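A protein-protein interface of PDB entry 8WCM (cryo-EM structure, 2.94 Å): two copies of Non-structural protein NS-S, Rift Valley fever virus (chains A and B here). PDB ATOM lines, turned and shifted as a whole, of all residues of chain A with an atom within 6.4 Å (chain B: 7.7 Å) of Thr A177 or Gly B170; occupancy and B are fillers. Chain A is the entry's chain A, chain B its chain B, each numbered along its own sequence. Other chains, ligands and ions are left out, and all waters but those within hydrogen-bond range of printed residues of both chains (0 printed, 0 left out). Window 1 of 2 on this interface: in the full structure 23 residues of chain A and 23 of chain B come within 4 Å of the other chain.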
ATOM      1  N   HIS A 172      -3.090 -11.171 -24.732  1.00  0.00           N
ATOM      2  CA  HIS A 172      -3.011  -9.725 -24.880  1.00  0.00           C
ATOM      3  C   HIS A 172      -2.721  -9.046 -23.551  1.00  0.00           C
ATOM      4  O   HIS A 172      -1.969  -8.068 -23.498  1.00  0.00           O
ATOM      5  CB  HIS A 172      -4.286  -9.163 -25.485  1.00  0.00           C
ATOM      6  CG  HIS A 172      -4.191  -7.706 -25.806  1.00  0.00           C
ATOM      7  ND1 HIS A 172      -4.989  -6.757 -25.208  1.00  0.00           N
ATOM      8  CD2 HIS A 172      -3.370  -7.032 -26.641  1.00  0.00           C
ATOM      9  CE1 HIS A 172      -4.673  -5.564 -25.672  1.00  0.00           C
ATOM     10  NE2 HIS A 172      -3.692  -5.703 -26.543  1.00  0.00           N
ATOM     11  N   ARG A 173      -3.317  -9.534 -22.466  1.00  0.00           N
ATOM     12  CA  ARG A 173      -3.056  -8.939 -21.162  1.00  0.00           C
ATOM     13  C   ARG A 173      -1.597  -9.101 -20.770  1.00  0.00           C
ATOM     14  O   ARG A 173      -0.999  -8.188 -20.192  1.00  0.00           O
ATOM     15  CB  ARG A 173      -3.972  -9.563 -20.118  1.00  0.00           C
ATOM     16  CG  ARG A 173      -5.421  -9.175 -20.261  1.00  0.00           C
ATOM     17  CD  ARG A 173      -6.179  -9.464 -19.001  1.00  0.00           C
ATOM     18  NE  ARG A 173      -5.469  -8.961 -17.837  1.00  0.00           N
ATOM     19  CZ  ARG A 173      -5.794  -7.854 -17.190  1.00  0.00           C
ATOM     20  NH1 ARG A 173      -6.821  -7.132 -17.591  1.00  0.00           N
ATOM     21  NH2 ARG A 173      -5.094  -7.473 -16.142  1.00  0.00           N
ATOM     22  N   MET A 174      -1.005 -10.256 -21.070  1.00  0.00           N
ATOM     23  CA  MET A 174       0.417 -10.462 -20.817  1.00  0.00           C
ATOM     24  C   MET A 174       1.270  -9.509 -21.638  1.00  0.00           C
ATOM     25  O   MET A 174       2.259  -8.958 -21.139  1.00  0.00           O
ATOM     26  CB  MET A 174       0.795 -11.903 -21.132  1.00  0.00           C
ATOM     27  CG  MET A 174       0.181 -12.926 -20.219  1.00  0.00           C
ATOM     28  SD  MET A 174       0.598 -14.599 -20.704  1.00  0.00           S
ATOM     29  CE  MET A 174       2.327 -14.631 -20.277  1.00  0.00           C
ATOM     30  N   ILE A 175       0.908  -9.313 -22.904  1.00  0.00           N
ATOM     31  CA  ILE A 175       1.645  -8.386 -23.758  1.00  0.00           C
ATOM     32  C   ILE A 175       1.622  -6.989 -23.163  1.00  0.00           C
ATOM     33  O   ILE A 175       2.650  -6.316 -23.078  1.00  0.00           O
ATOM     34  CB  ILE A 175       1.060  -8.387 -25.179  1.00  0.00           C
ATOM     35  CG1 ILE A 175       1.420  -9.667 -25.917  1.00  0.00           C
ATOM     36  CG2 ILE A 175       1.528  -7.187 -25.943  1.00  0.00           C
ATOM     37  CD1 ILE A 175       0.476  -9.964 -27.026  1.00  0.00           C
ATOM     38  N   VAL A 176       0.444  -6.530 -22.750  1.00  0.00           N
ATOM     39  CA  VAL A 176       0.332  -5.174 -22.225  1.00  0.00           C
ATOM     40  C   VAL A 176       1.047  -5.046 -20.887  1.00  0.00           C
ATOM     41  O   VAL A 176       1.617  -3.999 -20.576  1.00  0.00           O
ATOM     42  CB  VAL A 176      -1.142  -4.759 -22.130  1.00  0.00           C
ATOM     43  CG1 VAL A 176      -1.255  -3.391 -21.536  1.00  0.00           C
ATOM     44  CG2 VAL A 176      -1.761  -4.777 -23.491  1.00  0.00           C
ATOM     45  N   THR A 177       1.033  -6.098 -20.071  1.00  0.00           N
ATOM     46  CA  THR A 177       1.761  -6.047 -18.809  1.00  0.00           C
ATOM     47  C   THR A 177       3.254  -5.888 -19.049  1.00  0.00           C
ATOM     48  O   THR A 177       3.907  -5.042 -18.432  1.00  0.00           O
ATOM     49  CB  THR A 177       1.483  -7.301 -17.988  1.00  0.00           C
ATOM     50  OG1 THR A 177       0.073  -7.503 -17.884  1.00  0.00           O
ATOM     51  CG2 THR A 177       2.052  -7.155 -16.609  1.00  0.00           C
ATOM     52  N   GLU A 178       3.812  -6.685 -19.959  1.00  0.00           N
ATOM     53  CA  GLU A 178       5.231  -6.541 -20.260  1.00  0.00           C
ATOM     54  C   GLU A 178       5.547  -5.213 -20.931  1.00  0.00           C
ATOM     55  O   GLU A 178       6.618  -4.652 -20.704  1.00  0.00           O
ATOM     56  CB  GLU A 178       5.717  -7.692 -21.127  1.00  0.00           C
ATOM     57  CG  GLU A 178       7.222  -7.887 -21.099  1.00  0.00           C
ATOM     58  CD  GLU A 178       7.768  -8.367 -19.776  1.00  0.00           C
ATOM     59  OE1 GLU A 178       8.995  -8.562 -19.690  1.00  0.00           O
ATOM     60  OE2 GLU A 178       6.989  -8.574 -18.829  1.00  0.00           O
ATOM     61  N   ALA A 179       4.648  -4.700 -21.764  1.00  0.00           N
ATOM     62  CA  ALA A 179       4.868  -3.387 -22.351  1.00  0.00           C
ATOM     63  C   ALA A 179       4.930  -2.312 -21.283  1.00  0.00           C
ATOM     64  O   ALA A 179       5.788  -1.431 -21.328  1.00  0.00           O
ATOM     65  CB  ALA A 179       3.761  -3.073 -23.344  1.00  0.00           C
ATOM     66  N   ILE A 180       4.021  -2.363 -20.314  1.00  0.00           N
ATOM     67  CA  ILE A 180       4.026  -1.381 -19.237  1.00  0.00           C
ATOM     68  C   ILE A 180       5.304  -1.492 -18.423  1.00  0.00           C
ATOM     69  O   ILE A 180       5.913  -0.482 -18.058  1.00  0.00           O
ATOM     70  CB  ILE A 180       2.774  -1.555 -18.363  1.00  0.00           C
ATOM     71  CG1 ILE A 180       1.550  -1.018 -19.093  1.00  0.00           C
ATOM     72  CG2 ILE A 180       2.946  -0.860 -17.039  1.00  0.00           C
ATOM     73  CD1 ILE A 180       0.260  -1.455 -18.499  1.00  0.00           C
ATOM     74  N   LEU A 181       5.730  -2.718 -18.122  1.00  0.00           N
ATOM     75  CA  LEU A 181       6.940  -2.896 -17.328  1.00  0.00           C
ATOM     76  C   LEU A 181       8.177  -2.398 -18.063  1.00  0.00           C
ATOM     77  O   LEU A 181       9.028  -1.728 -17.472  1.00  0.00           O
ATOM     78  CB  LEU A 181       7.107  -4.361 -16.948  1.00  0.00           C
ATOM     79  CG  LEU A 181       6.026  -4.917 -16.036  1.00  0.00           C
ATOM     80  CD1 LEU A 181       6.254  -6.388 -15.829  1.00  0.00           C
ATOM     81  CD2 LEU A 181       6.032  -4.180 -14.730  1.00  0.00           C
ATOM     82  N   ARG A 182       8.294  -2.706 -19.349  1.00  0.00           N
ATOM     83  CA  ARG A 182       9.464  -2.338 -20.131  1.00  0.00           C
ATOM     84  C   ARG A 182       9.356  -0.959 -20.754  1.00  0.00           C
ATOM     85  O   ARG A 182      10.245  -0.571 -21.511  1.00  0.00           O
ATOM     86  CB  ARG A 182       9.708  -3.366 -21.232  1.00  0.00           C
ATOM     87  CG  ARG A 182       9.788  -4.781 -20.742  1.00  0.00           C
ATOM     88  CD  ARG A 182      11.155  -5.090 -20.202  1.00  0.00           C
ATOM     89  NE  ARG A 182      11.180  -6.378 -19.531  1.00  0.00           N
ATOM     90  CZ  ARG A 182      11.930  -6.647 -18.475  1.00  0.00           C
ATOM     91  NH1 ARG A 182      12.715  -5.714 -17.971  1.00  0.00           N
ATOM     92  NH2 ARG A 182      11.893  -7.846 -17.921  1.00  0.00           N
ATOM     93  N   LEU A 186       2.184   1.856 -25.723  1.00  0.00           N
ATOM     94  CA  LEU A 186       1.028   0.993 -25.921  1.00  0.00           C
ATOM     95  C   LEU A 186       0.213   1.354 -27.146  1.00  0.00           C
ATOM     96  O   LEU A 186      -0.724   0.631 -27.478  1.00  0.00           O
ATOM     97  CB  LEU A 186       0.119   1.016 -24.695  1.00  0.00           C
ATOM     98  CG  LEU A 186       0.630   0.336 -23.434  1.00  0.00           C
ATOM     99  CD1 LEU A 186      -0.335   0.574 -22.314  1.00  0.00           C
ATOM    100  CD2 LEU A 186       0.791  -1.128 -23.694  1.00  0.00           C
ATOM    101  N   PHE B  65      -8.528  -1.316  -8.289  1.00  0.00           N
ATOM    102  CA  PHE B  65      -7.239  -0.673  -8.502  1.00  0.00           C
ATOM    103  C   PHE B  65      -7.040  -0.354  -9.973  1.00  0.00           C
ATOM    104  O   PHE B  65      -6.465   0.678 -10.320  1.00  0.00           O
ATOM    105  CB  PHE B  65      -6.136  -1.585  -7.973  1.00  0.00           C
ATOM    106  CG  PHE B  65      -4.762  -0.997  -8.013  1.00  0.00           C
ATOM    107  CD1 PHE B  65      -4.559   0.360  -8.027  1.00  0.00           C
ATOM    108  CD2 PHE B  65      -3.662  -1.824  -8.015  1.00  0.00           C
ATOM    109  CE1 PHE B  65      -3.289   0.871  -8.065  1.00  0.00           C
ATOM    110  CE2 PHE B  65      -2.400  -1.312  -8.046  1.00  0.00           C
ATOM    111  CZ  PHE B  65      -2.213   0.033  -8.070  1.00  0.00           C
ATOM    112  N   TYR B  69      -5.276   2.917 -12.500  1.00  0.00           N
ATOM    113  CA  TYR B  69      -4.114   2.867 -13.369  1.00  0.00           C
ATOM    114  C   TYR B  69      -4.469   2.646 -14.829  1.00  0.00           C
ATOM    115  O   TYR B  69      -3.601   2.825 -15.685  1.00  0.00           O
ATOM    116  CB  TYR B  69      -3.124   1.801 -12.886  1.00  0.00           C
ATOM    117  CG  TYR B  69      -3.542   0.348 -12.981  1.00  0.00           C
ATOM    118  CD1 TYR B  69      -3.776  -0.260 -14.197  1.00  0.00           C
ATOM    119  CD2 TYR B  69      -3.633  -0.432 -11.849  1.00  0.00           C
ATOM    120  CE1 TYR B  69      -4.132  -1.573 -14.273  1.00  0.00           C
ATOM    121  CE2 TYR B  69      -3.980  -1.750 -11.921  1.00  0.00           C
ATOM    122  CZ  TYR B  69      -4.233  -2.312 -13.133  1.00  0.00           C
ATOM    123  OH  TYR B  69      -4.587  -3.632 -13.210  1.00  0.00           O
ATOM    124  N   PHE B  74      -3.455   6.852 -10.018  1.00  0.00           N
ATOM    125  CA  PHE B  74      -2.985   5.976  -8.989  1.00  0.00           C
ATOM    126  C   PHE B  74      -3.744   6.370  -7.734  1.00  0.00           C
ATOM    127  O   PHE B  74      -3.794   7.563  -7.413  1.00  0.00           O
ATOM    128  CB  PHE B  74      -1.484   6.105  -8.766  1.00  0.00           C
ATOM    129  CG  PHE B  74      -0.821   4.847  -8.300  1.00  0.00           C
ATOM    130  CD1 PHE B  74      -0.326   3.940  -9.204  1.00  0.00           C
ATOM    131  CD2 PHE B  74      -0.670   4.589  -6.959  1.00  0.00           C
ATOM    132  CE1 PHE B  74       0.295   2.802  -8.781  1.00  0.00           C
ATOM    133  CE2 PHE B  74      -0.052   3.448  -6.534  1.00  0.00           C
ATOM    134  CZ  PHE B  74       0.429   2.554  -7.447  1.00  0.00           C
ATOM    135  N   ALA B 154       6.731  -7.298  -4.926  1.00  0.00           N
ATOM    136  CA  ALA B 154       6.168  -6.638  -6.097  1.00  0.00           C
ATOM    137  C   ALA B 154       7.216  -6.469  -7.184  1.00  0.00           C
ATOM    138  O   ALA B 154       6.929  -6.673  -8.365  1.00  0.00           O
ATOM    139  CB  ALA B 154       5.578  -5.287  -5.712  1.00  0.00           C
ATOM    140  N   SER B 157       8.179 -10.014  -8.729  1.00  0.00           N
ATOM    141  CA  SER B 157       7.165 -10.556  -9.622  1.00  0.00           C
ATOM    142  C   SER B 157       7.348 -10.056 -11.045  1.00  0.00           C
ATOM    143  O   SER B 157       7.196 -10.824 -11.999  1.00  0.00           O
ATOM    144  CB  SER B 157       5.777 -10.179  -9.125  1.00  0.00           C
ATOM    145  OG  SER B 157       5.564 -10.675  -7.822  1.00  0.00           O
ATOM    146  N   CYS B 158       7.679  -8.777 -11.196  1.00  0.00           N
ATOM    147  CA  CYS B 158       7.762  -8.127 -12.494  1.00  0.00           C
ATOM    148  C   CYS B 158       9.133  -8.248 -13.139  1.00  0.00           C
ATOM    149  O   CYS B 158       9.244  -8.059 -14.353  1.00  0.00           O
ATOM    150  CB  CYS B 158       7.386  -6.657 -12.346  1.00  0.00           C
ATOM    151  SG  CYS B 158       5.754  -6.415 -11.646  1.00  0.00           S
ATOM    152  N   ILE B 160      11.819  -6.407 -13.036  1.00  0.00           N
ATOM    153  CA  ILE B 160      12.452  -5.176 -13.489  1.00  0.00           C
ATOM    154  C   ILE B 160      13.293  -4.623 -12.349  1.00  0.00           C
ATOM    155  O   ILE B 160      13.279  -5.161 -11.240  1.00  0.00           O
ATOM    156  CB  ILE B 160      11.401  -4.164 -13.969  1.00  0.00           C
ATOM    157  CG1 ILE B 160      10.404  -3.870 -12.857  1.00  0.00           C
ATOM    158  CG2 ILE B 160      10.678  -4.692 -15.175  1.00  0.00           C
ATOM    159  CD1 ILE B 160       9.454  -2.771 -13.193  1.00  0.00           C
ATOM    160  N   LEU B 164       8.933   1.394  -9.170  1.00  0.00           N
ATOM    161  CA  LEU B 164       8.171   0.721  -8.128  1.00  0.00           C
ATOM    162  C   LEU B 164       6.668   0.808  -8.348  1.00  0.00           C
ATOM    163  O   LEU B 164       5.956  -0.160  -8.079  1.00  0.00           O
ATOM    164  CB  LEU B 164       8.523   1.300  -6.758  1.00  0.00           C
ATOM    165  CG  LEU B 164       8.016   0.498  -5.563  1.00  0.00           C
ATOM    166  CD1 LEU B 164       8.631  -0.875  -5.563  1.00  0.00           C
ATOM    167  CD2 LEU B 164       8.328   1.215  -4.274  1.00  0.00           C
ATOM    168  N   GLU B 165       6.163   1.949  -8.814  1.00  0.00           N
ATOM    169  CA  GLU B 165       4.734   2.055  -9.086  1.00  0.00           C
ATOM    170  C   GLU B 165       4.326   1.140 -10.229  1.00  0.00           C
ATOM    171  O   GLU B 165       3.267   0.499 -10.181  1.00  0.00           O
ATOM    172  CB  GLU B 165       4.361   3.499  -9.395  1.00  0.00           C
ATOM    173  CG  GLU B 165       5.235   4.162 -10.426  1.00  0.00           C
ATOM    174  CD  GLU B 165       4.618   5.428 -10.960  1.00  0.00           C
ATOM    175  OE1 GLU B 165       3.419   5.404 -11.296  1.00  0.00           O
ATOM    176  OE2 GLU B 165       5.331   6.445 -11.047  1.00  0.00           O
ATOM    177  N   ASP B 166       5.150   1.065 -11.270  1.00  0.00           N
ATOM    178  CA  ASP B 166       4.878   0.123 -12.339  1.00  0.00           C
ATOM    179  C   ASP B 166       4.951  -1.311 -11.855  1.00  0.00           C
ATOM    180  O   ASP B 166       4.283  -2.170 -12.425  1.00  0.00           O
ATOM    181  CB  ASP B 166       5.845   0.329 -13.497  1.00  0.00           C
ATOM    182  CG  ASP B 166       5.440   1.474 -14.387  1.00  0.00           C
ATOM    183  OD1 ASP B 166       4.239   1.803 -14.421  1.00  0.00           O
ATOM    184  OD2 ASP B 166       6.316   2.035 -15.071  1.00  0.00           O
ATOM    185  N   SER B 167       5.723  -1.588 -10.808  1.00  0.00           N
ATOM    186  CA  SER B 167       5.753  -2.937 -10.260  1.00  0.00           C
ATOM    187  C   SER B 167       4.432  -3.300  -9.601  1.00  0.00           C
ATOM    188  O   SER B 167       3.952  -4.425  -9.750  1.00  0.00           O
ATOM    189  CB  SER B 167       6.898  -3.075  -9.270  1.00  0.00           C
ATOM    190  OG  SER B 167       8.133  -3.112  -9.953  1.00  0.00           O
ATOM    191  N   PHE B 168       3.824  -2.367  -8.874  1.00  0.00           N
ATOM    192  CA  PHE B 168       2.527  -2.648  -8.271  1.00  0.00           C
ATOM    193  C   PHE B 168       1.445  -2.775  -9.331  1.00  0.00           C
ATOM    194  O   PHE B 168       0.586  -3.663  -9.249  1.00  0.00           O
ATOM    195  CB  PHE B 168       2.175  -1.560  -7.264  1.00  0.00           C
ATOM    196  CG  PHE B 168       2.889  -1.706  -5.961  1.00  0.00           C
ATOM    197  CD1 PHE B 168       2.733  -2.846  -5.203  1.00  0.00           C
ATOM    198  CD2 PHE B 168       3.729  -0.721  -5.502  1.00  0.00           C
ATOM    199  CE1 PHE B 168       3.393  -2.989  -4.015  1.00  0.00           C
ATOM    200  CE2 PHE B 168       4.388  -0.867  -4.313  1.00  0.00           C
ATOM    201  CZ  PHE B 168       4.219  -1.999  -3.571  1.00  0.00           C
ATOM    202  N   VAL B 169       1.479  -1.908 -10.342  1.00  0.00           N
ATOM    203  CA  VAL B 169       0.524  -2.024 -11.437  1.00  0.00           C
ATOM    204  C   VAL B 169       0.689  -3.359 -12.149  1.00  0.00           C
ATOM    205  O   VAL B 169      -0.293  -4.038 -12.461  1.00  0.00           O
ATOM    206  CB  VAL B 169       0.679  -0.839 -12.402  1.00  0.00           C
ATOM    207  CG1 VAL B 169      -0.119  -1.072 -13.649  1.00  0.00           C
ATOM    208  CG2 VAL B 169       0.245   0.433 -11.726  1.00  0.00           C
ATOM    209  N   GLY B 170       1.931  -3.770 -12.397  1.00  0.00           N
ATOM    210  CA  GLY B 170       2.162  -5.036 -13.061  1.00  0.00           C
ATOM    211  C   GLY B 170       1.748  -6.226 -12.225  1.00  0.00           C
ATOM    212  O   GLY B 170       1.238  -7.211 -12.753  1.00  0.00           O
ATOM    213  N   LEU B 171       1.964  -6.159 -10.911  1.00  0.00           N
ATOM    214  CA  LEU B 171       1.541  -7.250 -10.043  1.00  0.00           C
ATOM    215  C   LEU B 171       0.027  -7.394 -10.036  1.00  0.00           C
ATOM    216  O   LEU B 171      -0.496  -8.511 -10.104  1.00  0.00           O
ATOM    217  CB  LEU B 171       2.061  -7.031  -8.627  1.00  0.00           C
ATOM    218  CG  LEU B 171       1.740  -8.153  -7.648  1.00  0.00           C
ATOM    219  CD1 LEU B 171       2.445  -9.413  -8.065  1.00  0.00           C
ATOM    220  CD2 LEU B 171       2.131  -7.765  -6.246  1.00  0.00           C
ATOM    221  N   HIS B 172      -0.700  -6.280  -9.966  1.00  0.00           N
ATOM    222  CA  HIS B 172      -2.150  -6.394 -10.031  1.00  0.00           C
ATOM    223  C   HIS B 172      -2.605  -6.911 -11.388  1.00  0.00           C
ATOM    224  O   HIS B 172      -3.552  -7.699 -11.472  1.00  0.00           O
ATOM    225  CB  HIS B 172      -2.820  -5.063  -9.730  1.00  0.00           C
ATOM    226  CG  HIS B 172      -4.307  -5.165  -9.627  1.00  0.00           C
ATOM    227  ND1 HIS B 172      -5.161  -4.507 -10.483  1.00  0.00           N
ATOM    228  CD2 HIS B 172      -5.093  -5.874  -8.786  1.00  0.00           C
ATOM    229  CE1 HIS B 172      -6.408  -4.795 -10.164  1.00  0.00           C
ATOM    230  NE2 HIS B 172      -6.394  -5.624  -9.139  1.00  0.00           N
ATOM    231  N   ARG B 173      -1.960  -6.468 -12.465  1.00  0.00           N
ATOM    232  CA  ARG B 173      -2.337  -6.950 -13.786  1.00  0.00           C
ATOM    233  C   ARG B 173      -2.094  -8.445 -13.914  1.00  0.00           C
ATOM    234  O   ARG B 173      -2.894  -9.158 -14.524  1.00  0.00           O
ATOM    235  CB  ARG B 173      -1.569  -6.181 -14.853  1.00  0.00           C
ATOM    236  CG  ARG B 173      -1.995  -4.744 -15.003  1.00  0.00           C
ATOM    237  CD  ARG B 173      -1.521  -4.177 -16.306  1.00  0.00           C
ATOM    238  NE  ARG B 173      -1.822  -5.076 -17.407  1.00  0.00           N
ATOM    239  CZ  ARG B 173      -2.817  -4.898 -18.260  1.00  0.00           C
ATOM    240  NH1 ARG B 173      -3.608  -3.851 -18.142  1.00  0.00           N
ATOM    241  NH2 ARG B 173      -3.018  -5.765 -19.231  1.00  0.00           N
ATOM    242  N   MET B 174      -0.992  -8.938 -13.350  1.00  0.00           N
ATOM    243  CA  MET B 174      -0.727 -10.373 -13.340  1.00  0.00           C
ATOM    244  C   MET B 174      -1.786 -11.126 -12.552  1.00  0.00           C
ATOM    245  O   MET B 174      -2.236 -12.202 -12.968  1.00  0.00           O
ATOM    246  CB  MET B 174       0.650 -10.641 -12.751  1.00  0.00           C
ATOM    247  CG  MET B 174       1.796 -10.134 -13.580  1.00  0.00           C
ATOM    248  SD  MET B 174       3.378 -10.406 -12.783  1.00  0.00           S
ATOM    249  CE  MET B 174       3.501 -12.177 -12.922  1.00  0.00           C
ATOM    250  N   ILE B 175      -2.186 -10.582 -11.405  1.00  0.00           N
ATOM    251  CA  ILE B 175      -3.226 -11.214 -10.599  1.00  0.00           C
ATOM    252  C   ILE B 175      -4.511 -11.338 -11.399  1.00  0.00           C
ATOM    253  O   ILE B 175      -5.147 -12.393 -11.424  1.00  0.00           O
ATOM    254  CB  ILE B 175      -3.459 -10.419  -9.305  1.00  0.00           C
ATOM    255  CG1 ILE B 175      -2.307 -10.611  -8.331  1.00  0.00           C
ATOM    256  CG2 ILE B 175      -4.758 -10.812  -8.671  1.00  0.00           C
ATOM    257  CD1 ILE B 175      -2.204  -9.497  -7.352  1.00  0.00           C
ATOM    258  N   VAL B 176      -4.916 -10.257 -12.057  1.00  0.00           N
ATOM    259  CA  VAL B 176      -6.173 -10.279 -12.796  1.00  0.00           C
ATOM    260  C   VAL B 176      -6.076 -11.196 -14.009  1.00  0.00           C
ATOM    261  O   VAL B 176      -7.053 -11.848 -14.385  1.00  0.00           O
ATOM    262  CB  VAL B 176      -6.588  -8.856 -13.186  1.00  0.00           C
ATOM    263  CG1 VAL B 176      -7.847  -8.889 -13.994  1.00  0.00           C
ATOM    264  CG2 VAL B 176      -6.796  -8.034 -11.954  1.00  0.00           C
ATOM    265  N   THR B 177      -4.908 -11.265 -14.645  1.00  0.00           N
ATOM    266  CA  THR B 177      -4.748 -12.181 -15.770  1.00  0.00           C
ATOM    267  C   THR B 177      -4.921 -13.623 -15.323  1.00  0.00           C
ATOM    268  O   THR B 177      -5.649 -14.397 -15.954  1.00  0.00           O
ATOM    269  CB  THR B 177      -3.384 -11.984 -16.419  1.00  0.00           C
ATOM    270  OG1 THR B 177      -3.188 -10.599 -16.712  1.00  0.00           O
ATOM    271  CG2 THR B 177      -3.300 -12.763 -17.698  1.00  0.00           C
ATOM    272  N   LEU B 194      -2.792  -6.512  -2.107  1.00  0.00           N
ATOM    273  CA  LEU B 194      -2.237  -7.282  -3.218  1.00  0.00           C
ATOM    274  C   LEU B 194      -1.623  -8.600  -2.773  1.00  0.00           C
ATOM    275  O   LEU B 194      -1.678  -9.591  -3.510  1.00  0.00           O
ATOM    276  CB  LEU B 194      -1.200  -6.446  -3.961  1.00  0.00           C
ATOM    277  CG  LEU B 194      -1.759  -5.382  -4.897  1.00  0.00           C
ATOM    278  CD1 LEU B 194      -0.639  -4.649  -5.578  1.00  0.00           C
ATOM    279  CD2 LEU B 194      -2.669  -6.017  -5.913  1.00  0.00           C
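The guanidinium group of Arg A173 sits at hydrogen-bond distance from the backbone carbonyl oxygen of Arg B173 (3.2 Å). The guanidinium group (NE) of Arg A173 is in hydrogen-bond range of the side-chain hydroxyl (OG1) of Thr B177, 3.0 Å away. The side-chain hydroxyl of Thr A177 is in hydrogen-bond range of the guanidinium group of Arg B173 (3.1 Å).
The backbone carbonyl oxygen of Ala B154 sits at hydrogen-bond distance from the side-chain sulfur of Cys B158, 3.5 Å away. NE of Arg A182 lies within salt-bridge range of OE1 of Glu A178 (3.1 Å). The backbone carbonyl oxygen (O) of Arg B173 lies within hydrogen-bond range of the side-chain hydroxyl (OG1) of Thr B177 (2.6 Å). The side-chain sulfur (SG) of Cys B158 sits at hydrogen-bond distance from the backbone carbonyl oxygen (O) of Ser B167, 3.3 Å away. The backbone carbonyl oxygen (O) of Arg A173 is in hydrogen-bond range of the side-chain hydroxyl (OG1) of Thr A177 (2.6 Å).
Among the printed residues, merely in contact across the chains: Leu A181 with Asp B166, Arg A173 with Val B176, Val A176 with Arg B173, Arg A182 with Ile B160, Leu A181 with Cys B158, Ile A180 with Arg B173, Ile A180 with Asp B166 and Thr A177 with Gly B170.
Of chain B, only Gly B170 (3.9 Å) and Arg B173 (3.1 Å) come within 4 Å of Thr A177. Of the printed residues of chain B, Ile A180 touches Asp B166 (3.9 Å) and Arg B173 (3.9 Å). Of the printed residues of chain B, Arg A182 touches Ile B160 (3.6 Å). Met B174 touches none of the printed residues of chain A. The nearest residue of chain B that does not touch Thr A177 is Met B174 (4.3 Å). The nearest residue of chain A that does not touch Gly B170 is Leu A181 (4.3 Å). The nearest printed residue of chain A that does not touch Val B176 is Thr A177 (8.2 Å).
Of the 22 printed residues of chain B, 7 touch a printed residue of chain A. Hydrophobic or aromatic side chains of chain B within 4 Å of the printed part of chain A: Ile B160 and Val B176. Hydrophobic or aromatic side chains of chain A within 4 Å of the printed part of chain B: Val A176, Ile A180 and Leu A181. Along chain A the printed residues that touch a printed residue of chain B span positions 173 to 182. Among the printed residues, 11 pairs touch across the chains. Among the printed residues, no Asp or Glu carboxylate lies within 4 Å of a Lys or Arg side-chain nitrogen of the other chain.
Arg A173 touches its own counterpart, Arg B173. Arg A173 touches Val B176, and with the chains exchanged Val A176 touches Arg B173. Arg A173 touches Thr B177, and with the chains exchanged Thr A177 touches Arg B173.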
